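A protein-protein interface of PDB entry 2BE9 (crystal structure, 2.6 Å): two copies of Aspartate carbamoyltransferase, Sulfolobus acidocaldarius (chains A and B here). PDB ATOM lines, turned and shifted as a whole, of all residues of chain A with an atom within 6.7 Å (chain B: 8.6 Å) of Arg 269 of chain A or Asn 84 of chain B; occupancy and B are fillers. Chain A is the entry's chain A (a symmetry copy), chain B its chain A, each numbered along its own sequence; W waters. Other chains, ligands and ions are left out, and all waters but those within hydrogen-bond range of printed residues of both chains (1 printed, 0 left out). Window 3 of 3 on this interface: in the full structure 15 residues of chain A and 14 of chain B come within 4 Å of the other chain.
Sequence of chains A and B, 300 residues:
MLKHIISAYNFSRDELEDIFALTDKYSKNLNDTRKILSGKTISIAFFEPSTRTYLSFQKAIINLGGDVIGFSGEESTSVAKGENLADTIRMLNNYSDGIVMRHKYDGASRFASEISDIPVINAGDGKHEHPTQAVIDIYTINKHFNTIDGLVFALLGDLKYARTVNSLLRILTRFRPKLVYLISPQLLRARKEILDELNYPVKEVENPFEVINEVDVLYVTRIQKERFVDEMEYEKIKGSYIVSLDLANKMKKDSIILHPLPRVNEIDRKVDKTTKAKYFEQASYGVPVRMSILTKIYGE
Of the printed residues of chain B, Arg 263 of chain A touches Asp 87.
Of chain B, only Asn 84 (2.4 Å) and Asp 87 (3.4 Å) come within 4 Å of Arg 269 of chain A.
Of the printed residues of chain B, Phe 280 of chain A touches Asp 87 (3.6 Å) and Arg 90 (3.6 Å).
Of the printed residues of chain A, Gly 82 of chain B touches Val 264 (3.998 Å).
Glu 83 of chain B touches none of the printed residues of chain A.
Printed residues of chain A within 4 Å of Asn 84 of chain B: Arg 269.
Printed residues of chain A within 4 Å of Arg 90 of chain B: Phe 280 (3.6 Å).
The nearest residue of chain B that does not touch Arg 269 of chain A is Arg 90 of chain B (4.5 Å).
Water W1 lies within hydrogen-bond range of N of Arg 263 of chain A, OD1 of Asp 87 of chain B and OE1 of Glu 83 of chain B.
No position is printed for both chains.
Of the 6 pairs that touch across the chains among the printed residues, none has its exchanged pair printed and touching as well.
The side-chain amide oxygen of Asn 84 of chain B sits at hydrogen-bond distance from the guanidinium group of Arg 269 of chain A (2.4 Å).
OD2 of Asp 87 of chain B is in salt-bridge range of NH1 of Arg 263 of chain A.
OD1 of Asp 87 of chain B lies within salt-bridge range of NH2 of Arg 269 of chain A, at 3.4 Å.
Among the printed residues, merely in contact across the chains: Val 264 of chain A with Gly 82 of chain B (3.998 Å), Phe 280 of chain A with Asp 87 of chain B (3.6 Å) and Phe 280 of chain A with Arg 90 of chain B (3.6 Å).
Of the 14 printed residues of chain B, 4 touch a printed residue of chain A.
Hydrophobic or aromatic side chains of chain A that line the printed part of chain B: Val 264 and Phe 280.
The backbone carbonyl oxygen (O) of Asn 84 of chain B lies within hydrogen-bond range of the side-chain hydroxyl (OG1) of Thr 88 of chain B (3.0 Å).
The guanidinium group of Arg 90 of chain B is in salt-bridge range of the side-chain carboxylate of Asp 87 of chain B (2.8 Å).
NH2 of Arg 263 of chain A lies within salt-bridge range of OD2 of Asp 272 of chain A (2.9 Å).
NH1 of Arg 269 of chain A lies within hydrogen-bond range of O of Val 264 of chain A (3.2 Å).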
ATOM      1  N   VAL A 243      21.931  -9.777 -13.934  1.00  0.00           N
ATOM      2  CA  VAL A 243      21.193  -9.428 -12.726  1.00  0.00           C
ATOM      3  C   VAL A 243      21.648 -10.381 -11.610  1.00  0.00           C
ATOM      4  O   VAL A 243      21.290 -11.576 -11.603  1.00  0.00           O
ATOM      5  CB  VAL A 243      19.647  -9.464 -12.923  1.00  0.00           C
ATOM      6  CG1 VAL A 243      18.943  -9.088 -11.646  1.00  0.00           C
ATOM      7  CG2 VAL A 243      19.228  -8.516 -14.012  1.00  0.00           C
ATOM      8  N   ARG A 263      15.472 -17.290 -20.330  1.00  0.00           N
ATOM      9  CA  ARG A 263      16.743 -16.766 -19.849  1.00  0.00           C
ATOM     10  C   ARG A 263      17.753 -17.858 -20.104  1.00  0.00           C
ATOM     11  O   ARG A 263      17.387 -19.016 -20.283  1.00  0.00           O
ATOM     12  CB  ARG A 263      16.722 -16.435 -18.344  1.00  0.00           C
ATOM     13  CG  ARG A 263      15.710 -17.232 -17.523  1.00  0.00           C
ATOM     14  CD  ARG A 263      16.319 -18.000 -16.391  1.00  0.00           C
ATOM     15  NE  ARG A 263      16.098 -17.410 -15.067  1.00  0.00           N
ATOM     16  CZ  ARG A 263      15.470 -18.011 -14.050  1.00  0.00           C
ATOM     17  NH1 ARG A 263      14.930 -19.212 -14.167  1.00  0.00           N
ATOM     18  NH2 ARG A 263      15.367 -17.389 -12.895  1.00  0.00           N
ATOM     19  N   VAL A 264      19.022 -17.474 -20.148  1.00  0.00           N
ATOM     20  CA  VAL A 264      20.114 -18.425 -20.059  1.00  0.00           C
ATOM     21  C   VAL A 264      20.816 -18.234 -18.693  1.00  0.00           C
ATOM     22  O   VAL A 264      20.460 -18.898 -17.721  1.00  0.00           O
ATOM     23  CB  VAL A 264      21.084 -18.307 -21.268  1.00  0.00           C
ATOM     24  CG1 VAL A 264      22.189 -19.374 -21.196  1.00  0.00           C
ATOM     25  CG2 VAL A 264      20.298 -18.392 -22.586  1.00  0.00           C
ATOM     26  N   ASN A 265      21.760 -17.293 -18.629  1.00  0.00           N
ATOM     27  CA  ASN A 265      22.533 -17.037 -17.421  1.00  0.00           C
ATOM     28  C   ASN A 265      22.571 -15.577 -17.009  1.00  0.00           C
ATOM     29  O   ASN A 265      23.335 -15.201 -16.105  1.00  0.00           O
ATOM     30  CB  ASN A 265      23.969 -17.543 -17.600  1.00  0.00           C
ATOM     31  CG  ASN A 265      24.093 -19.029 -17.350  1.00  0.00           C
ATOM     32  OD1 ASN A 265      24.755 -19.728 -18.105  1.00  0.00           O
ATOM     33  ND2 ASN A 265      23.451 -19.522 -16.292  1.00  0.00           N
ATOM     34  N   ILE A 267      20.313 -13.810 -15.518  1.00  0.00           N
ATOM     35  CA  ILE A 267      19.782 -13.582 -14.180  1.00  0.00           C
ATOM     36  C   ILE A 267      20.327 -14.674 -13.272  1.00  0.00           C
ATOM     37  O   ILE A 267      20.188 -15.859 -13.570  1.00  0.00           O
ATOM     38  CB  ILE A 267      18.215 -13.599 -14.124  1.00  0.00           C
ATOM     39  CG1 ILE A 267      17.606 -12.528 -15.017  1.00  0.00           C
ATOM     40  CG2 ILE A 267      17.710 -13.384 -12.712  1.00  0.00           C
ATOM     41  CD1 ILE A 267      16.097 -12.689 -15.193  1.00  0.00           C
ATOM     42  N   ASP A 268      20.962 -14.259 -12.177  1.00  0.00           N
ATOM     43  CA  ASP A 268      21.313 -15.147 -11.082  1.00  0.00           C
ATOM     44  C   ASP A 268      20.027 -15.784 -10.547  1.00  0.00           C
ATOM     45  O   ASP A 268      19.076 -15.081 -10.189  1.00  0.00           O
ATOM     46  CB  ASP A 268      22.008 -14.323  -9.989  1.00  0.00           C
ATOM     47  CG  ASP A 268      22.615 -15.179  -8.870  1.00  0.00           C
ATOM     48  OD1 ASP A 268      23.271 -14.584  -7.981  1.00  0.00           O
ATOM     49  OD2 ASP A 268      22.449 -16.422  -8.852  1.00  0.00           O
ATOM     50  N   ARG A 269      20.006 -17.115 -10.484  1.00  0.00           N
ATOM     51  CA  ARG A 269      18.794 -17.871 -10.094  1.00  0.00           C
ATOM     52  C   ARG A 269      18.367 -17.688  -8.648  1.00  0.00           C
ATOM     53  O   ARG A 269      17.265 -18.100  -8.260  1.00  0.00           O
ATOM     54  CB  ARG A 269      18.942 -19.356 -10.436  1.00  0.00           C
ATOM     55  CG  ARG A 269      19.368 -19.534 -11.867  1.00  0.00           C
ATOM     56  CD  ARG A 269      18.939 -20.825 -12.491  1.00  0.00           C
ATOM     57  NE  ARG A 269      19.121 -20.716 -13.940  1.00  0.00           N
ATOM     58  CZ  ARG A 269      18.173 -20.904 -14.859  1.00  0.00           C
ATOM     59  NH1 ARG A 269      18.475 -20.765 -16.140  1.00  0.00           N
ATOM     60  NH2 ARG A 269      16.942 -21.247 -14.509  1.00  0.00           N
ATOM     61  N   LYS A 270      19.226 -17.067  -7.846  1.00  0.00           N
ATOM     62  CA  LYS A 270      18.859 -16.786  -6.456  1.00  0.00           C
ATOM     63  C   LYS A 270      17.832 -15.647  -6.393  1.00  0.00           C
ATOM     64  O   LYS A 270      17.012 -15.595  -5.462  1.00  0.00           O
ATOM     65  CB  LYS A 270      20.081 -16.455  -5.611  1.00  0.00           C
ATOM     66  CG  LYS A 270      20.855 -17.665  -5.108  1.00  0.00           C
ATOM     67  CD  LYS A 270      22.046 -17.220  -4.252  1.00  0.00           C
ATOM     68  CE  LYS A 270      23.041 -18.350  -4.059  1.00  0.00           C
ATOM     69  NZ  LYS A 270      22.340 -19.565  -3.541  1.00  0.00           N
ATOM     70  N   VAL A 271      17.878 -14.766  -7.401  1.00  0.00           N
ATOM     71  CA  VAL A 271      16.921 -13.669  -7.562  1.00  0.00           C
ATOM     72  C   VAL A 271      15.472 -14.178  -7.574  1.00  0.00           C
ATOM     73  O   VAL A 271      14.579 -13.530  -7.001  1.00  0.00           O
ATOM     74  CB  VAL A 271      17.214 -12.855  -8.847  1.00  0.00           C
ATOM     75  CG1 VAL A 271      16.261 -11.670  -8.979  1.00  0.00           C
ATOM     76  CG2 VAL A 271      18.668 -12.392  -8.874  1.00  0.00           C
ATOM     77  N   ASP A 272      15.267 -15.340  -8.204  1.00  0.00           N
ATOM     78  CA  ASP A 272      13.978 -16.038  -8.246  1.00  0.00           C
ATOM     79  C   ASP A 272      13.245 -16.016  -6.928  1.00  0.00           C
ATOM     80  O   ASP A 272      12.033 -15.845  -6.897  1.00  0.00           O
ATOM     81  CB  ASP A 272      14.150 -17.508  -8.639  1.00  0.00           C
ATOM     82  CG  ASP A 272      14.637 -17.685 -10.058  1.00  0.00           C
ATOM     83  OD1 ASP A 272      15.003 -16.675 -10.698  1.00  0.00           O
ATOM     84  OD2 ASP A 272      14.663 -18.842 -10.527  1.00  0.00           O
ATOM     85  N   LYS A 273      13.982 -16.201  -5.842  1.00  0.00           N
ATOM     86  CA  LYS A 273      13.371 -16.341  -4.513  1.00  0.00           C
ATOM     87  C   LYS A 273      13.067 -15.005  -3.822  1.00  0.00           C
ATOM     88  O   LYS A 273      12.324 -14.978  -2.853  1.00  0.00           O
ATOM     89  CB  LYS A 273      14.192 -17.296  -3.625  1.00  0.00           C
ATOM     90  CG  LYS A 273      14.465 -18.660  -4.305  1.00  0.00           C
ATOM     91  CD  LYS A 273      14.321 -19.889  -3.374  1.00  0.00           C
ATOM     92  CE  LYS A 273      15.181 -19.809  -2.079  1.00  0.00           C
ATOM     93  NZ  LYS A 273      16.653 -19.574  -2.311  1.00  0.00           N
ATOM     94  N   TYR A 279       9.493 -11.985 -13.370  1.00  0.00           N
ATOM     95  CA  TYR A 279       9.553 -12.548 -14.734  1.00  0.00           C
ATOM     96  C   TYR A 279       8.672 -13.794 -14.892  1.00  0.00           C
ATOM     97  O   TYR A 279       8.140 -14.046 -15.974  1.00  0.00           O
ATOM     98  CB  TYR A 279      11.004 -12.814 -15.202  1.00  0.00           C
ATOM     99  CG  TYR A 279      11.969 -13.162 -14.087  1.00  0.00           C
ATOM    100  CD1 TYR A 279      12.627 -12.157 -13.381  1.00  0.00           C
ATOM    101  CD2 TYR A 279      12.217 -14.493 -13.734  1.00  0.00           C
ATOM    102  CE1 TYR A 279      13.494 -12.451 -12.354  1.00  0.00           C
ATOM    103  CE2 TYR A 279      13.083 -14.804 -12.696  1.00  0.00           C
ATOM    104  CZ  TYR A 279      13.724 -13.766 -12.004  1.00  0.00           C
ATOM    105  OH  TYR A 279      14.595 -14.032 -10.966  1.00  0.00           O
ATOM    106  N   PHE A 280       8.503 -14.562 -13.822  1.00  0.00           N
ATOM    107  CA  PHE A 280       7.603 -15.711 -13.863  1.00  0.00           C
ATOM    108  C   PHE A 280       6.130 -15.289 -13.904  1.00  0.00           C
ATOM    109  O   PHE A 280       5.318 -15.881 -14.623  1.00  0.00           O
ATOM    110  CB  PHE A 280       7.909 -16.683 -12.717  1.00  0.00           C
ATOM    111  CG  PHE A 280       9.220 -17.411 -12.891  1.00  0.00           C
ATOM    112  CD1 PHE A 280       9.571 -17.966 -14.135  1.00  0.00           C
ATOM    113  CD2 PHE A 280      10.091 -17.580 -11.818  1.00  0.00           C
ATOM    114  CE1 PHE A 280      10.781 -18.642 -14.315  1.00  0.00           C
ATOM    115  CE2 PHE A 280      11.304 -18.263 -11.979  1.00  0.00           C
ATOM    116  CZ  PHE A 280      11.655 -18.783 -13.224  1.00  0.00           C
ATOM    117  N   PHE B  47      11.003 -33.691 -25.564  1.00  0.00           N
ATOM    118  CA  PHE B  47      12.323 -33.091 -25.788  1.00  0.00           C
ATOM    119  C   PHE B  47      13.154 -34.030 -26.614  1.00  0.00           C
ATOM    120  O   PHE B  47      13.927 -33.598 -27.457  1.00  0.00           O
ATOM    121  CB  PHE B  47      13.043 -32.827 -24.483  1.00  0.00           C
ATOM    122  CG  PHE B  47      12.344 -31.871 -23.604  1.00  0.00           C
ATOM    123  CD1 PHE B  47      11.325 -32.301 -22.790  1.00  0.00           C
ATOM    124  CD2 PHE B  47      12.709 -30.537 -23.593  1.00  0.00           C
ATOM    125  CE1 PHE B  47      10.650 -31.419 -21.969  1.00  0.00           C
ATOM    126  CE2 PHE B  47      12.049 -29.626 -22.778  1.00  0.00           C
ATOM    127  CZ  PHE B  47      11.018 -30.069 -21.954  1.00  0.00           C
ATOM    128  N   GLY B  82      19.566 -21.678 -24.742  1.00  0.00           N
ATOM    129  CA  GLY B  82      19.842 -22.766 -23.793  1.00  0.00           C
ATOM    130  C   GLY B  82      18.996 -22.698 -22.514  1.00  0.00           C
ATOM    131  O   GLY B  82      19.545 -22.554 -21.388  1.00  0.00           O
ATOM    132  N   GLU B  83      17.669 -22.784 -22.693  1.00  0.00           N
ATOM    133  CA  GLU B  83      16.745 -22.853 -21.579  1.00  0.00           C
ATOM    134  C   GLU B  83      16.792 -24.183 -20.857  1.00  0.00           C
ATOM    135  O   GLU B  83      16.652 -25.239 -21.450  1.00  0.00           O
ATOM    136  CB  GLU B  83      15.321 -22.545 -22.027  1.00  0.00           C
ATOM    137  CG  GLU B  83      14.230 -23.009 -21.063  1.00  0.00           C
ATOM    138  CD  GLU B  83      12.851 -22.467 -21.432  1.00  0.00           C
ATOM    139  OE1 GLU B  83      12.575 -21.281 -21.103  1.00  0.00           O
ATOM    140  OE2 GLU B  83      12.060 -23.235 -22.048  1.00  0.00           O
ATOM    141  N   ASN B  84      17.123 -24.077 -19.584  1.00  0.00           N
ATOM    142  CA  ASN B  84      16.692 -24.897 -18.462  1.00  0.00           C
ATOM    143  C   ASN B  84      15.480 -25.836 -18.611  1.00  0.00           C
ATOM    144  O   ASN B  84      14.410 -25.392 -19.045  1.00  0.00           O
ATOM    145  CB  ASN B  84      16.270 -23.866 -17.400  1.00  0.00           C
ATOM    146  CG  ASN B  84      16.652 -24.264 -16.032  1.00  0.00           C
ATOM    147  OD1 ASN B  84      16.375 -23.556 -15.085  1.00  0.00           O
ATOM    148  ND2 ASN B  84      17.319 -25.386 -15.904  1.00  0.00           N
ATOM    149  N   LEU B  85      15.601 -27.086 -18.162  1.00  0.00           N
ATOM    150  CA  LEU B  85      14.409 -27.925 -18.013  1.00  0.00           C
ATOM    151  C   LEU B  85      13.432 -27.291 -17.016  1.00  0.00           C
ATOM    152  O   LEU B  85      12.225 -27.184 -17.297  1.00  0.00           O
ATOM    153  CB  LEU B  85      14.735 -29.343 -17.563  1.00  0.00           C
ATOM    154  CG  LEU B  85      13.829 -30.528 -17.961  1.00  0.00           C
ATOM    155  CD1 LEU B  85      13.755 -31.588 -16.858  1.00  0.00           C
ATOM    156  CD2 LEU B  85      12.417 -30.188 -18.442  1.00  0.00           C
ATOM    157  N   ALA B  86      13.950 -26.860 -15.866  1.00  0.00           N
ATOM    158  CA  ALA B  86      13.105 -26.227 -14.857  1.00  0.00           C
ATOM    159  C   ALA B  86      12.246 -25.114 -15.467  1.00  0.00           C
ATOM    160  O   ALA B  86      11.025 -25.156 -15.360  1.00  0.00           O
ATOM    161  CB  ALA B  86      13.937 -25.726 -13.691  1.00  0.00           C
ATOM    162  N   ASP B  87      12.863 -24.159 -16.152  1.00  0.00           N
ATOM    163  CA  ASP B  87      12.116 -23.062 -16.775  1.00  0.00           C
ATOM    164  C   ASP B  87      11.065 -23.551 -17.759  1.00  0.00           C
ATOM    165  O   ASP B  87       9.956 -22.996 -17.835  1.00  0.00           O
ATOM    166  CB  ASP B  87      13.057 -22.056 -17.440  1.00  0.00           C
ATOM    167  CG  ASP B  87      13.735 -21.133 -16.436  1.00  0.00           C
ATOM    168  OD1 ASP B  87      14.617 -20.353 -16.845  1.00  0.00           O
ATOM    169  OD2 ASP B  87      13.390 -21.168 -15.228  1.00  0.00           O
ATOM    170  N   THR B  88      11.395 -24.594 -18.507  1.00  0.00           N
ATOM    171  CA  THR B  88      10.446 -25.165 -19.432  1.00  0.00           C
ATOM    172  C   THR B  88       9.257 -25.727 -18.670  1.00  0.00           C
ATOM    173  O   THR B  88       8.107 -25.500 -19.059  1.00  0.00           O
ATOM    174  CB  THR B  88      11.101 -26.241 -20.319  1.00  0.00           C
ATOM    175  OG1 THR B  88      12.179 -25.637 -21.029  1.00  0.00           O
ATOM    176  CG2 THR B  88      10.125 -26.785 -21.342  1.00  0.00           C
ATOM    177  N   ILE B  89       9.528 -26.437 -17.575  1.00  0.00           N
ATOM    178  CA  ILE B  89       8.445 -27.015 -16.795  1.00  0.00           C
ATOM    179  C   ILE B  89       7.545 -25.922 -16.201  1.00  0.00           C
ATOM    180  O   ILE B  89       6.307 -26.058 -16.221  1.00  0.00           O
ATOM    181  CB  ILE B  89       8.938 -28.026 -15.745  1.00  0.00           C
ATOM    182  CG1 ILE B  89       9.683 -29.206 -16.413  1.00  0.00           C
ATOM    183  CG2 ILE B  89       7.797 -28.517 -14.890  1.00  0.00           C
ATOM    184  CD1 ILE B  89       8.927 -30.034 -17.459  1.00  0.00           C
ATOM    185  N   ARG B  90       8.155 -24.825 -15.737  1.00  0.00           N
ATOM    186  CA  ARG B  90       7.377 -23.687 -15.218  1.00  0.00           C
ATOM    187  C   ARG B  90       6.457 -23.100 -16.287  1.00  0.00           C
ATOM    188  O   ARG B  90       5.325 -22.728 -15.990  1.00  0.00           O
ATOM    189  CB  ARG B  90       8.275 -22.592 -14.643  1.00  0.00           C
ATOM    190  CG  ARG B  90       8.885 -22.917 -13.295  1.00  0.00           C
ATOM    191  CD  ARG B  90      10.095 -22.041 -12.966  1.00  0.00           C
ATOM    192  NE  ARG B  90      10.826 -22.570 -11.814  1.00  0.00           N
ATOM    193  CZ  ARG B  90      12.144 -22.773 -11.765  1.00  0.00           C
ATOM    194  NH1 ARG B  90      12.929 -22.472 -12.800  1.00  0.00           N
ATOM    195  NH2 ARG B  90      12.688 -23.289 -10.670  1.00  0.00           N
ATOM    196  N   MET B  91       6.949 -23.038 -17.524  1.00  0.00           N
ATOM    197  CA  MET B  91       6.188 -22.535 -18.665  1.00  0.00           C
ATOM    198  C   MET B  91       4.986 -23.448 -18.929  1.00  0.00           C
ATOM    199  O   MET B  91       3.853 -22.961 -19.069  1.00  0.00           O
ATOM    200  CB  MET B  91       7.102 -22.396 -19.888  1.00  0.00           C
ATOM    201  CG  MET B  91       6.417 -22.251 -21.260  1.00  0.00           C
ATOM    202  SD  MET B  91       7.456 -22.789 -22.690  1.00  0.00           S
ATOM    203  CE  MET B  91       7.270 -24.573 -22.588  1.00  0.00           C
ATOM    204  N   HIS B 103      12.398 -37.357 -22.363  1.00  0.00           N
ATOM    205  CA  HIS B 103      13.647 -36.587 -22.296  1.00  0.00           C
ATOM    206  C   HIS B 103      14.879 -37.508 -22.371  1.00  0.00           C
ATOM    207  O   HIS B 103      14.842 -38.646 -21.908  1.00  0.00           O
ATOM    208  CB  HIS B 103      13.657 -35.815 -20.981  1.00  0.00           C
ATOM    209  CG  HIS B 103      14.436 -34.545 -21.019  1.00  0.00           C
ATOM    210  ND1 HIS B 103      15.814 -34.515 -20.988  1.00  0.00           N
ATOM    211  CD2 HIS B 103      14.030 -33.254 -21.052  1.00  0.00           C
ATOM    212  CE1 HIS B 103      16.224 -33.258 -21.023  1.00  0.00           C
ATOM    213  NE2 HIS B 103      15.161 -32.474 -21.068  1.00  0.00           N
ATOM    214  N   PHE B 111      12.719 -34.839 -11.674  1.00  0.00           N
ATOM    215  CA  PHE B 111      13.011 -33.441 -11.426  1.00  0.00           C
ATOM    216  C   PHE B 111      11.837 -32.560 -11.860  1.00  0.00           C
ATOM    217  O   PHE B 111      11.412 -31.668 -11.116  1.00  0.00           O
ATOM    218  CB  PHE B 111      14.336 -33.014 -12.096  1.00  0.00           C
ATOM    219  CG  PHE B 111      14.637 -31.549 -11.966  1.00  0.00           C
ATOM    220  CD1 PHE B 111      14.641 -30.723 -13.091  1.00  0.00           C
ATOM    221  CD2 PHE B 111      14.887 -30.977 -10.713  1.00  0.00           C
ATOM    222  CE1 PHE B 111      14.901 -29.343 -12.977  1.00  0.00           C
ATOM    223  CE2 PHE B 111      15.157 -29.596 -10.583  1.00  0.00           C
ATOM    224  CZ  PHE B 111      15.163 -28.781 -11.722  1.00  0.00           C
ATOM    225  N   ILE B 115       9.448 -29.667  -9.717  1.00  0.00           N
ATOM    226  CA  ILE B 115       9.250 -28.259 -10.049  1.00  0.00           C
ATOM    227  C   ILE B 115       7.771 -27.959 -10.239  1.00  0.00           C
ATOM    228  O   ILE B 115       7.324 -26.856  -9.996  1.00  0.00           O
ATOM    229  CB  ILE B 115      10.010 -27.885 -11.347  1.00  0.00           C
ATOM    230  CG1 ILE B 115      11.510 -28.129 -11.168  1.00  0.00           C
ATOM    231  CG2 ILE B 115       9.761 -26.409 -11.764  1.00  0.00           C
ATOM    232  CD1 ILE B 115      12.203 -27.248 -10.053  1.00  0.00           C
HETATM  233  O   HOH W   1      13.693 -19.151 -19.377  1.00  0.00           O
